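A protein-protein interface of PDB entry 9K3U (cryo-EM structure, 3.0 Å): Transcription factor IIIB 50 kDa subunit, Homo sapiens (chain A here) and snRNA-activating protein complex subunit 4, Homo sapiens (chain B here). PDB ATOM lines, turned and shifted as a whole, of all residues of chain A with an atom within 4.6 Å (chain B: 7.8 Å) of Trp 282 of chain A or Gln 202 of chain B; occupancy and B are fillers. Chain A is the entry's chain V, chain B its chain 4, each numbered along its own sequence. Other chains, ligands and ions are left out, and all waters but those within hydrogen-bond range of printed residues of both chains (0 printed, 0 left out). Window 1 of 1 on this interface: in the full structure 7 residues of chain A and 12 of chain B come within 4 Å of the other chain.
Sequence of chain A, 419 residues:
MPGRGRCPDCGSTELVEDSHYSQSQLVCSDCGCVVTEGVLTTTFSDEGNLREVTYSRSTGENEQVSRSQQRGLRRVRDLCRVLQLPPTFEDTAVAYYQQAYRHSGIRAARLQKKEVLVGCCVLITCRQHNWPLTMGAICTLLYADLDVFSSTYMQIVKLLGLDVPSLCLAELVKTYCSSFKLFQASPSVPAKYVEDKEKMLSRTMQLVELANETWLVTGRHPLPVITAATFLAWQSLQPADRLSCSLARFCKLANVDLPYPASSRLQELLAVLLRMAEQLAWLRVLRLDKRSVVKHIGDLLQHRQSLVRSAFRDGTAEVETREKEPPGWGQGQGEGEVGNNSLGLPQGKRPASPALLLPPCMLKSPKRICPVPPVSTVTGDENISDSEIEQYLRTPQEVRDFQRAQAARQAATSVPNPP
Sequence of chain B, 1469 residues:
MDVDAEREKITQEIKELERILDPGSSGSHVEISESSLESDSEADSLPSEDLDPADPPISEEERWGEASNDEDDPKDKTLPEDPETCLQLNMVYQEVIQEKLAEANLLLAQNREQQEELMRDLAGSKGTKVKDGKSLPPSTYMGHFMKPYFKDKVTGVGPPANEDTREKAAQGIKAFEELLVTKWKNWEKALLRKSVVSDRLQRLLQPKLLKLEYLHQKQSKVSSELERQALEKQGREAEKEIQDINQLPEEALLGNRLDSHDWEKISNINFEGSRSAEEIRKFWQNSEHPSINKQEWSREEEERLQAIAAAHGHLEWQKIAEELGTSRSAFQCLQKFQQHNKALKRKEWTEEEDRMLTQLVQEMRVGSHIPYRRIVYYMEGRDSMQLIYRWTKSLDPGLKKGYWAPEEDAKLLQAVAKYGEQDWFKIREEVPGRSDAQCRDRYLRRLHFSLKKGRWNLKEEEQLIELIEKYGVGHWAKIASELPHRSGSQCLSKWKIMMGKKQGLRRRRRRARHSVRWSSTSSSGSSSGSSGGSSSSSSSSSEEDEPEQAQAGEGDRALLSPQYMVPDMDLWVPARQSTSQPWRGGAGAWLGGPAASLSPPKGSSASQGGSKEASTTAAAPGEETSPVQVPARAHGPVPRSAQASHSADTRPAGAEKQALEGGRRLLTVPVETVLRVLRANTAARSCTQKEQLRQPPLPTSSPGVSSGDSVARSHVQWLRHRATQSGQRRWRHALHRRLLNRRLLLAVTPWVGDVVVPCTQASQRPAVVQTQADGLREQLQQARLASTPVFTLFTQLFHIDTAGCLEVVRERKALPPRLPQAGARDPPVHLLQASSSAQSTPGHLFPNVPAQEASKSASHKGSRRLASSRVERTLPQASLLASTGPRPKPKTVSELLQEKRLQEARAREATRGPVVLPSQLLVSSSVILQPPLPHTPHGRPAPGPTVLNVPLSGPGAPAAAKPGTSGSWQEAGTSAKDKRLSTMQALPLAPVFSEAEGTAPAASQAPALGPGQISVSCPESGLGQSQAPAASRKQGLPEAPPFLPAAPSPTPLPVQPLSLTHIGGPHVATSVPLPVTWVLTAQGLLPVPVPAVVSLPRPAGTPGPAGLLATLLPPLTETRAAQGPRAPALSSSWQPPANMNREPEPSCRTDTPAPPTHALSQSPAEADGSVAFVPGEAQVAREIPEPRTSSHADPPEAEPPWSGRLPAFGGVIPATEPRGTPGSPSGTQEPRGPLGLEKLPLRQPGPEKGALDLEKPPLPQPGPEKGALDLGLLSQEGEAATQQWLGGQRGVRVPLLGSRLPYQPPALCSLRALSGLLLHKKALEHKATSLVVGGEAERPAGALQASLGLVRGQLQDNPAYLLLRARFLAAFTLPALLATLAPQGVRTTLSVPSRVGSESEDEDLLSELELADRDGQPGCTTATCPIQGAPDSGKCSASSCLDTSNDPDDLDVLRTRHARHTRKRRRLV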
ATOM      1  N   LEU A 280      -4.289 -15.137 -24.764  1.00  0.00           N
ATOM      2  CA  LEU A 280      -3.402 -16.291 -24.797  1.00  0.00           C
ATOM      3  C   LEU A 280      -4.174 -17.564 -24.470  1.00  0.00           C
ATOM      4  O   LEU A 280      -5.261 -17.522 -23.891  1.00  0.00           O
ATOM      5  CB  LEU A 280      -2.243 -16.110 -23.817  1.00  0.00           C
ATOM      6  CG  LEU A 280      -1.058 -15.275 -24.314  1.00  0.00           C
ATOM      7  CD1 LEU A 280      -0.031 -15.114 -23.212  1.00  0.00           C
ATOM      8  CD2 LEU A 280      -0.418 -15.904 -25.545  1.00  0.00           C
ATOM      9  N   ALA A 281      -3.599 -18.707 -24.852  1.00  0.00           N
ATOM     10  CA  ALA A 281      -4.312 -19.975 -24.740  1.00  0.00           C
ATOM     11  C   ALA A 281      -4.204 -20.557 -23.335  1.00  0.00           C
ATOM     12  O   ALA A 281      -5.217 -20.784 -22.664  1.00  0.00           O
ATOM     13  CB  ALA A 281      -3.771 -20.966 -25.775  1.00  0.00           C
ATOM     14  N   TRP A 282      -2.979 -20.815 -22.871  1.00  0.00           N
ATOM     15  CA  TRP A 282      -2.814 -21.503 -21.594  1.00  0.00           C
ATOM     16  C   TRP A 282      -3.307 -20.649 -20.431  1.00  0.00           C
ATOM     17  O   TRP A 282      -3.850 -21.179 -19.453  1.00  0.00           O
ATOM     18  CB  TRP A 282      -1.351 -21.898 -21.393  1.00  0.00           C
ATOM     19  CG  TRP A 282      -0.385 -20.756 -21.447  1.00  0.00           C
ATOM     20  CD1 TRP A 282       0.047 -19.999 -20.399  1.00  0.00           C
ATOM     21  CD2 TRP A 282       0.279 -20.244 -22.610  1.00  0.00           C
ATOM     22  NE1 TRP A 282       0.934 -19.046 -20.835  1.00  0.00           N
ATOM     23  CE2 TRP A 282       1.093 -19.174 -22.191  1.00  0.00           C
ATOM     24  CE3 TRP A 282       0.261 -20.587 -23.966  1.00  0.00           C
ATOM     25  CZ2 TRP A 282       1.882 -18.444 -23.076  1.00  0.00           C
ATOM     26  CZ3 TRP A 282       1.045 -19.860 -24.844  1.00  0.00           C
ATOM     27  CH2 TRP A 282       1.845 -18.801 -24.396  1.00  0.00           C
ATOM     28  N   LEU A 283      -3.145 -19.326 -20.519  1.00  0.00           N
ATOM     29  CA  LEU A 283      -3.562 -18.467 -19.415  1.00  0.00           C
ATOM     30  C   LEU A 283      -5.079 -18.395 -19.308  1.00  0.00           C
ATOM     31  O   LEU A 283      -5.631 -18.417 -18.200  1.00  0.00           O
ATOM     32  CB  LEU A 283      -2.969 -17.069 -19.581  1.00  0.00           C
ATOM     33  CG  LEU A 283      -1.440 -16.973 -19.590  1.00  0.00           C
ATOM     34  CD1 LEU A 283      -1.000 -15.529 -19.734  1.00  0.00           C
ATOM     35  CD2 LEU A 283      -0.841 -17.584 -18.332  1.00  0.00           C
ATOM     36  N   ARG A 284      -5.778 -18.304 -20.444  1.00  0.00           N
ATOM     37  CA  ARG A 284      -7.234 -18.282 -20.404  1.00  0.00           C
ATOM     38  C   ARG A 284      -7.806 -19.592 -19.880  1.00  0.00           C
ATOM     39  O   ARG A 284      -8.935 -19.605 -19.378  1.00  0.00           O
ATOM     40  CB  ARG A 284      -7.800 -17.982 -21.795  1.00  0.00           C
ATOM     41  CG  ARG A 284      -8.064 -19.211 -22.653  1.00  0.00           C
ATOM     42  CD  ARG A 284      -8.302 -18.835 -24.107  1.00  0.00           C
ATOM     43  NE  ARG A 284      -9.478 -17.985 -24.272  1.00  0.00           N
ATOM     44  CZ  ARG A 284      -9.895 -17.503 -25.440  1.00  0.00           C
ATOM     45  NH1 ARG A 284      -9.234 -17.782 -26.555  1.00  0.00           N
ATOM     46  NH2 ARG A 284     -10.978 -16.739 -25.492  1.00  0.00           N
ATOM     47  N   VAL A 285      -7.055 -20.691 -19.984  1.00  0.00           N
ATOM     48  CA  VAL A 285      -7.482 -21.946 -19.379  1.00  0.00           C
ATOM     49  C   VAL A 285      -7.159 -21.957 -17.892  1.00  0.00           C
ATOM     50  O   VAL A 285      -7.945 -22.451 -17.077  1.00  0.00           O
ATOM     51  CB  VAL A 285      -6.827 -23.135 -20.108  1.00  0.00           C
ATOM     52  CG1 VAL A 285      -7.166 -24.443 -19.401  1.00  0.00           C
ATOM     53  CG2 VAL A 285      -7.266 -23.172 -21.569  1.00  0.00           C
ATOM     54  N   LEU A 286      -5.999 -21.412 -17.512  1.00  0.00           N
ATOM     55  CA  LEU A 286      -5.669 -21.282 -16.098  1.00  0.00           C
ATOM     56  C   LEU A 286      -6.670 -20.407 -15.356  1.00  0.00           C
ATOM     57  O   LEU A 286      -6.879 -20.603 -14.154  1.00  0.00           O
ATOM     58  CB  LEU A 286      -4.264 -20.701 -15.934  1.00  0.00           C
ATOM     59  CG  LEU A 286      -3.088 -21.590 -16.345  1.00  0.00           C
ATOM     60  CD1 LEU A 286      -1.778 -20.827 -16.226  1.00  0.00           C
ATOM     61  CD2 LEU A 286      -3.048 -22.855 -15.506  1.00  0.00           C
ATOM     62  N   GLN A 302       6.221 -11.228 -24.048  1.00  0.00           N
ATOM     63  CA  GLN A 302       7.035 -11.927 -25.037  1.00  0.00           C
ATOM     64  C   GLN A 302       6.475 -11.741 -26.440  1.00  0.00           C
ATOM     65  O   GLN A 302       7.235 -11.513 -27.392  1.00  0.00           O
ATOM     66  CB  GLN A 302       7.120 -13.413 -24.685  1.00  0.00           C
ATOM     67  CG  GLN A 302       8.086 -14.203 -25.555  1.00  0.00           C
ATOM     68  CD  GLN A 302       8.124 -15.675 -25.196  1.00  0.00           C
ATOM     69  OE1 GLN A 302       7.452 -16.115 -24.262  1.00  0.00           O
ATOM     70  NE2 GLN A 302       8.913 -16.446 -25.937  1.00  0.00           N
ATOM     71  N   LYS B 194      -2.903 -27.891 -13.166  1.00  0.00           N
ATOM     72  CA  LYS B 194      -3.024 -26.733 -14.043  1.00  0.00           C
ATOM     73  C   LYS B 194      -1.654 -26.204 -14.451  1.00  0.00           C
ATOM     74  O   LYS B 194      -1.438 -25.858 -15.617  1.00  0.00           O
ATOM     75  CB  LYS B 194      -3.839 -25.639 -13.354  1.00  0.00           C
ATOM     76  CG  LYS B 194      -5.310 -25.979 -13.182  1.00  0.00           C
ATOM     77  CD  LYS B 194      -6.056 -24.864 -12.466  1.00  0.00           C
ATOM     78  CE  LYS B 194      -7.536 -25.182 -12.323  1.00  0.00           C
ATOM     79  NZ  LYS B 194      -8.210 -25.331 -13.642  1.00  0.00           N
ATOM     80  N   SER B 195      -0.716 -26.135 -13.503  1.00  0.00           N
ATOM     81  CA  SER B 195       0.613 -25.629 -13.811  1.00  0.00           C
ATOM     82  C   SER B 195       1.340 -26.544 -14.785  1.00  0.00           C
ATOM     83  O   SER B 195       1.997 -26.066 -15.715  1.00  0.00           O
ATOM     84  CB  SER B 195       1.423 -25.466 -12.524  1.00  0.00           C
ATOM     85  OG  SER B 195       1.521 -26.693 -11.824  1.00  0.00           O
ATOM     86  N   VAL B 196       1.239 -27.860 -14.590  1.00  0.00           N
ATOM     87  CA  VAL B 196       1.896 -28.785 -15.508  1.00  0.00           C
ATOM     88  C   VAL B 196       1.309 -28.649 -16.908  1.00  0.00           C
ATOM     89  O   VAL B 196       2.046 -28.589 -17.904  1.00  0.00           O
ATOM     90  CB  VAL B 196       1.783 -30.231 -14.987  1.00  0.00           C
ATOM     91  CG1 VAL B 196       2.402 -31.202 -15.984  1.00  0.00           C
ATOM     92  CG2 VAL B 196       2.445 -30.360 -13.621  1.00  0.00           C
ATOM     93  N   VAL B 197      -0.021 -28.588 -17.006  1.00  0.00           N
ATOM     94  CA  VAL B 197      -0.657 -28.463 -18.317  1.00  0.00           C
ATOM     95  C   VAL B 197      -0.242 -27.163 -18.989  1.00  0.00           C
ATOM     96  O   VAL B 197       0.082 -27.137 -20.185  1.00  0.00           O
ATOM     97  CB  VAL B 197      -2.188 -28.565 -18.177  1.00  0.00           C
ATOM     98  CG1 VAL B 197      -2.868 -28.271 -19.508  1.00  0.00           C
ATOM     99  CG2 VAL B 197      -2.581 -29.943 -17.663  1.00  0.00           C
ATOM    100  N   SER B 198      -0.244 -26.059 -18.237  1.00  0.00           N
ATOM    101  CA  SER B 198       0.119 -24.770 -18.811  1.00  0.00           C
ATOM    102  C   SER B 198       1.578 -24.755 -19.251  1.00  0.00           C
ATOM    103  O   SER B 198       1.900 -24.219 -20.316  1.00  0.00           O
ATOM    104  CB  SER B 198      -0.147 -23.653 -17.804  1.00  0.00           C
ATOM    105  OG  SER B 198       0.573 -23.866 -16.602  1.00  0.00           O
ATOM    106  N   ASP B 199       2.470 -25.337 -18.450  1.00  0.00           N
ATOM    107  CA  ASP B 199       3.881 -25.383 -18.823  1.00  0.00           C
ATOM    108  C   ASP B 199       4.076 -26.191 -20.096  1.00  0.00           C
ATOM    109  O   ASP B 199       4.817 -25.783 -20.998  1.00  0.00           O
ATOM    110  CB  ASP B 199       4.703 -25.970 -17.674  1.00  0.00           C
ATOM    111  CG  ASP B 199       6.196 -25.783 -17.869  1.00  0.00           C
ATOM    112  OD1 ASP B 199       6.651 -25.726 -19.031  1.00  0.00           O
ATOM    113  OD2 ASP B 199       6.922 -25.694 -16.854  1.00  0.00           O
ATOM    114  N   ARG B 200       3.414 -27.346 -20.194  1.00  0.00           N
ATOM    115  CA  ARG B 200       3.535 -28.161 -21.397  1.00  0.00           C
ATOM    116  C   ARG B 200       3.020 -27.409 -22.619  1.00  0.00           C
ATOM    117  O   ARG B 200       3.684 -27.364 -23.664  1.00  0.00           O
ATOM    118  CB  ARG B 200       2.780 -29.480 -21.215  1.00  0.00           C
ATOM    119  CG  ARG B 200       2.794 -30.391 -22.439  1.00  0.00           C
ATOM    120  CD  ARG B 200       4.210 -30.742 -22.872  1.00  0.00           C
ATOM    121  NE  ARG B 200       4.225 -31.665 -24.003  1.00  0.00           N
ATOM    122  CZ  ARG B 200       5.329 -32.098 -24.603  1.00  0.00           C
ATOM    123  NH1 ARG B 200       6.521 -31.694 -24.185  1.00  0.00           N
ATOM    124  NH2 ARG B 200       5.243 -32.938 -25.625  1.00  0.00           N
ATOM    125  N   LEU B 201       1.835 -26.802 -22.504  1.00  0.00           N
ATOM    126  CA  LEU B 201       1.266 -26.089 -23.643  1.00  0.00           C
ATOM    127  C   LEU B 201       2.139 -24.908 -24.046  1.00  0.00           C
ATOM    128  O   LEU B 201       2.321 -24.638 -25.238  1.00  0.00           O
ATOM    129  CB  LEU B 201      -0.154 -25.625 -23.313  1.00  0.00           C
ATOM    130  CG  LEU B 201      -0.927 -24.940 -24.443  1.00  0.00           C
ATOM    131  CD1 LEU B 201      -0.969 -25.816 -25.688  1.00  0.00           C
ATOM    132  CD2 LEU B 201      -2.336 -24.595 -23.989  1.00  0.00           C
ATOM    133  N   GLN B 202       2.706 -24.200 -23.065  1.00  0.00           N
ATOM    134  CA  GLN B 202       3.553 -23.053 -23.377  1.00  0.00           C
ATOM    135  C   GLN B 202       4.847 -23.494 -24.044  1.00  0.00           C
ATOM    136  O   GLN B 202       5.306 -22.854 -24.998  1.00  0.00           O
ATOM    137  CB  GLN B 202       3.840 -22.259 -22.100  1.00  0.00           C
ATOM    138  CG  GLN B 202       4.711 -21.024 -22.303  1.00  0.00           C
ATOM    139  CD  GLN B 202       6.198 -21.333 -22.260  1.00  0.00           C
ATOM    140  OE1 GLN B 202       6.606 -22.454 -21.957  1.00  0.00           O
ATOM    141  NE2 GLN B 202       7.017 -20.333 -22.565  1.00  0.00           N
ATOM    142  N   ARG B 203       5.457 -24.577 -23.559  1.00  0.00           N
ATOM    143  CA  ARG B 203       6.682 -25.065 -24.182  1.00  0.00           C
ATOM    144  C   ARG B 203       6.414 -25.607 -25.580  1.00  0.00           C
ATOM    145  O   ARG B 203       7.308 -25.582 -26.434  1.00  0.00           O
ATOM    146  CB  ARG B 203       7.328 -26.138 -23.307  1.00  0.00           C
ATOM    147  CG  ARG B 203       8.703 -26.580 -23.783  1.00  0.00           C
ATOM    148  CD  ARG B 203       8.644 -27.881 -24.568  1.00  0.00           C
ATOM    149  NE  ARG B 203       8.335 -29.021 -23.709  1.00  0.00           N
ATOM    150  CZ  ARG B 203       9.234 -29.691 -22.993  1.00  0.00           C
ATOM    151  NH1 ARG B 203      10.512 -29.337 -23.020  1.00  0.00           N
ATOM    152  NH2 ARG B 203       8.853 -30.715 -22.243  1.00  0.00           N
ATOM    153  N   LEU B 204       5.198 -26.099 -25.831  1.00  0.00           N
ATOM    154  CA  LEU B 204       4.861 -26.563 -27.174  1.00  0.00           C
ATOM    155  C   LEU B 204       4.561 -25.399 -28.114  1.00  0.00           C
ATOM    156  O   LEU B 204       4.861 -25.473 -29.310  1.00  0.00           O
ATOM    157  CB  LEU B 204       3.662 -27.513 -27.115  1.00  0.00           C
ATOM    158  CG  LEU B 204       3.908 -28.882 -26.471  1.00  0.00           C
ATOM    159  CD1 LEU B 204       2.604 -29.652 -26.353  1.00  0.00           C
ATOM    160  CD2 LEU B 204       4.932 -29.678 -27.266  1.00  0.00           C
ATOM    161  N   LEU B 205       3.975 -24.318 -27.593  1.00  0.00           N
ATOM    162  CA  LEU B 205       3.556 -23.215 -28.453  1.00  0.00           C
ATOM    163  C   LEU B 205       4.667 -22.197 -28.685  1.00  0.00           C
ATOM    164  O   LEU B 205       4.659 -21.514 -29.717  1.00  0.00           O
ATOM    165  CB  LEU B 205       2.336 -22.516 -27.849  1.00  0.00           C
ATOM    166  CG  LEU B 205       1.039 -23.330 -27.815  1.00  0.00           C
ATOM    167  CD1 LEU B 205      -0.046 -22.567 -27.072  1.00  0.00           C
ATOM    168  CD2 LEU B 205       0.578 -23.681 -29.222  1.00  0.00           C
ATOM    169  N   GLN B 206       5.619 -22.071 -27.761  1.00  0.00           N
ATOM    170  CA  GLN B 206       6.660 -21.058 -27.917  1.00  0.00           C
ATOM    171  C   GLN B 206       7.420 -21.206 -29.225  1.00  0.00           C
ATOM    172  O   GLN B 206       7.631 -20.191 -29.913  1.00  0.00           O
ATOM    173  CB  GLN B 206       7.601 -21.099 -26.709  1.00  0.00           C
ATOM    174  CG  GLN B 206       8.718 -20.064 -26.752  1.00  0.00           C
ATOM    175  CD  GLN B 206       9.578 -20.082 -25.503  1.00  0.00           C
ATOM    176  OE1 GLN B 206       9.347 -20.872 -24.588  1.00  0.00           O
ATOM    177  NE2 GLN B 206      10.577 -19.209 -25.459  1.00  0.00           N
ATOM    178  N   PRO B 207       7.859 -22.403 -29.634  1.00  0.00           N
ATOM    179  CA  PRO B 207       8.479 -22.514 -30.965  1.00  0.00           C
ATOM    180  C   PRO B 207       7.535 -22.109 -32.083  1.00  0.00           C
ATOM    181  O   PRO B 207       7.953 -21.446 -33.039  1.00  0.00           O
ATOM    182  CB  PRO B 207       8.866 -23.999 -31.051  1.00  0.00           C
ATOM    183  CG  PRO B 207       8.890 -24.482 -29.640  1.00  0.00           C
ATOM    184  CD  PRO B 207       7.843 -23.693 -28.924  1.00  0.00           C
ATOM    185  N   LYS B 208       6.258 -22.480 -31.974  1.00  0.00           N
ATOM    186  CA  LYS B 208       5.292 -22.106 -33.002  1.00  0.00           C
ATOM    187  C   LYS B 208       5.069 -20.598 -33.018  1.00  0.00           C
ATOM    188  O   LYS B 208       4.934 -19.995 -34.089  1.00  0.00           O
ATOM    189  CB  LYS B 208       3.973 -22.842 -32.769  1.00  0.00           C
ATOM    190  CG  LYS B 208       3.083 -22.959 -34.004  1.00  0.00           C
ATOM    191  CD  LYS B 208       3.693 -23.844 -35.092  1.00  0.00           C
ATOM    192  CE  LYS B 208       3.885 -25.280 -34.621  1.00  0.00           C
ATOM    193  NZ  LYS B 208       4.368 -26.167 -35.716  1.00  0.00           N
ATOM    194  N   LEU B 209       5.030 -19.968 -31.841  1.00  0.00           N
ATOM    195  CA  LEU B 209       4.883 -18.518 -31.790  1.00  0.00           C
ATOM    196  C   LEU B 209       6.095 -17.821 -32.398  1.00  0.00           C
ATOM    197  O   LEU B 209       5.948 -16.830 -33.125  1.00  0.00           O
ATOM    198  CB  LEU B 209       4.670 -18.061 -30.346  1.00  0.00           C
ATOM    199  CG  LEU B 209       3.366 -18.506 -29.680  1.00  0.00           C
ATOM    200  CD1 LEU B 209       3.324 -18.047 -28.231  1.00  0.00           C
ATOM    201  CD2 LEU B 209       2.155 -17.982 -30.441  1.00  0.00           C
ATOM    202  N   LYS B 265      11.140 -24.266 -11.735  1.00  0.00           N
ATOM    203  CA  LYS B 265      10.411 -23.158 -12.343  1.00  0.00           C
ATOM    204  C   LYS B 265       8.939 -23.201 -11.958  1.00  0.00           C
ATOM    205  O   LYS B 265       8.376 -22.204 -11.487  1.00  0.00           O
ATOM    206  CB  LYS B 265      10.581 -23.210 -13.862  1.00  0.00           C
ATOM    207  CG  LYS B 265       9.748 -22.206 -14.645  1.00  0.00           C
ATOM    208  CD  LYS B 265       8.639 -22.902 -15.425  1.00  0.00           C
ATOM    209  CE  LYS B 265       8.010 -21.981 -16.460  1.00  0.00           C
ATOM    210  NZ  LYS B 265       6.972 -22.680 -17.266  1.00  0.00           N
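Among the printed residues, merely in contact across the chains: Leu 286 of chain A with Lys 194 of chain B, Leu 286 of chain A with Ser 198 of chain B, Trp 282 of chain A with Leu 205 of chain B, Trp 282 of chain A with Leu 201 of chain B and Trp 282 of chain A with Gln 202 of chain B.
NE2 of Gln 302 of chain A lies close to NE2 of Gln 206 of chain B (3.3 Å).
Of the 8 printed residues of chain A, 3 touch a printed residue of chain B.
Along chain A the printed residues that touch a printed residue of chain B span positions 282 to 302.
Printed residues of chain B that touch a printed residue of chain A: Lys 194, Ser 198, Leu 201, Gln 202, Leu 205 and Gln 206.
Among the printed residues, no Asp or Glu carboxylate lies within 4 Å of a Lys or Arg side-chain nitrogen of the other chain.
Trp 282 of chain A touches three residues of chain B.
Printed residues of chain B within 4 Å of Leu 286 of chain A: Lys 194 (3.4 Å) and Ser 198 (3.6 Å).
Gln 202 of chain B touches one residue of chain A.
Printed residues of chain A within 4 Å of Gln 206 of chain B: Gln 302.
The nearest printed residue of chain B that does not touch Gln 302 of chain A is Gln 202 of chain B (4.6 Å).
OG of Ser 198 of chain B lies within hydrogen-bond range of O of Lys 194 of chain B (3.0 Å).
The side-chain hydroxyl (OG) of Ser 198 of chain B lies within hydrogen-bond range of the backbone carbonyl oxygen (O) of Ser 195 of chain B (2.8 Å).
NE2 of Gln 202 of chain B lies within hydrogen-bond range of OE1 of Gln 206 of chain B.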
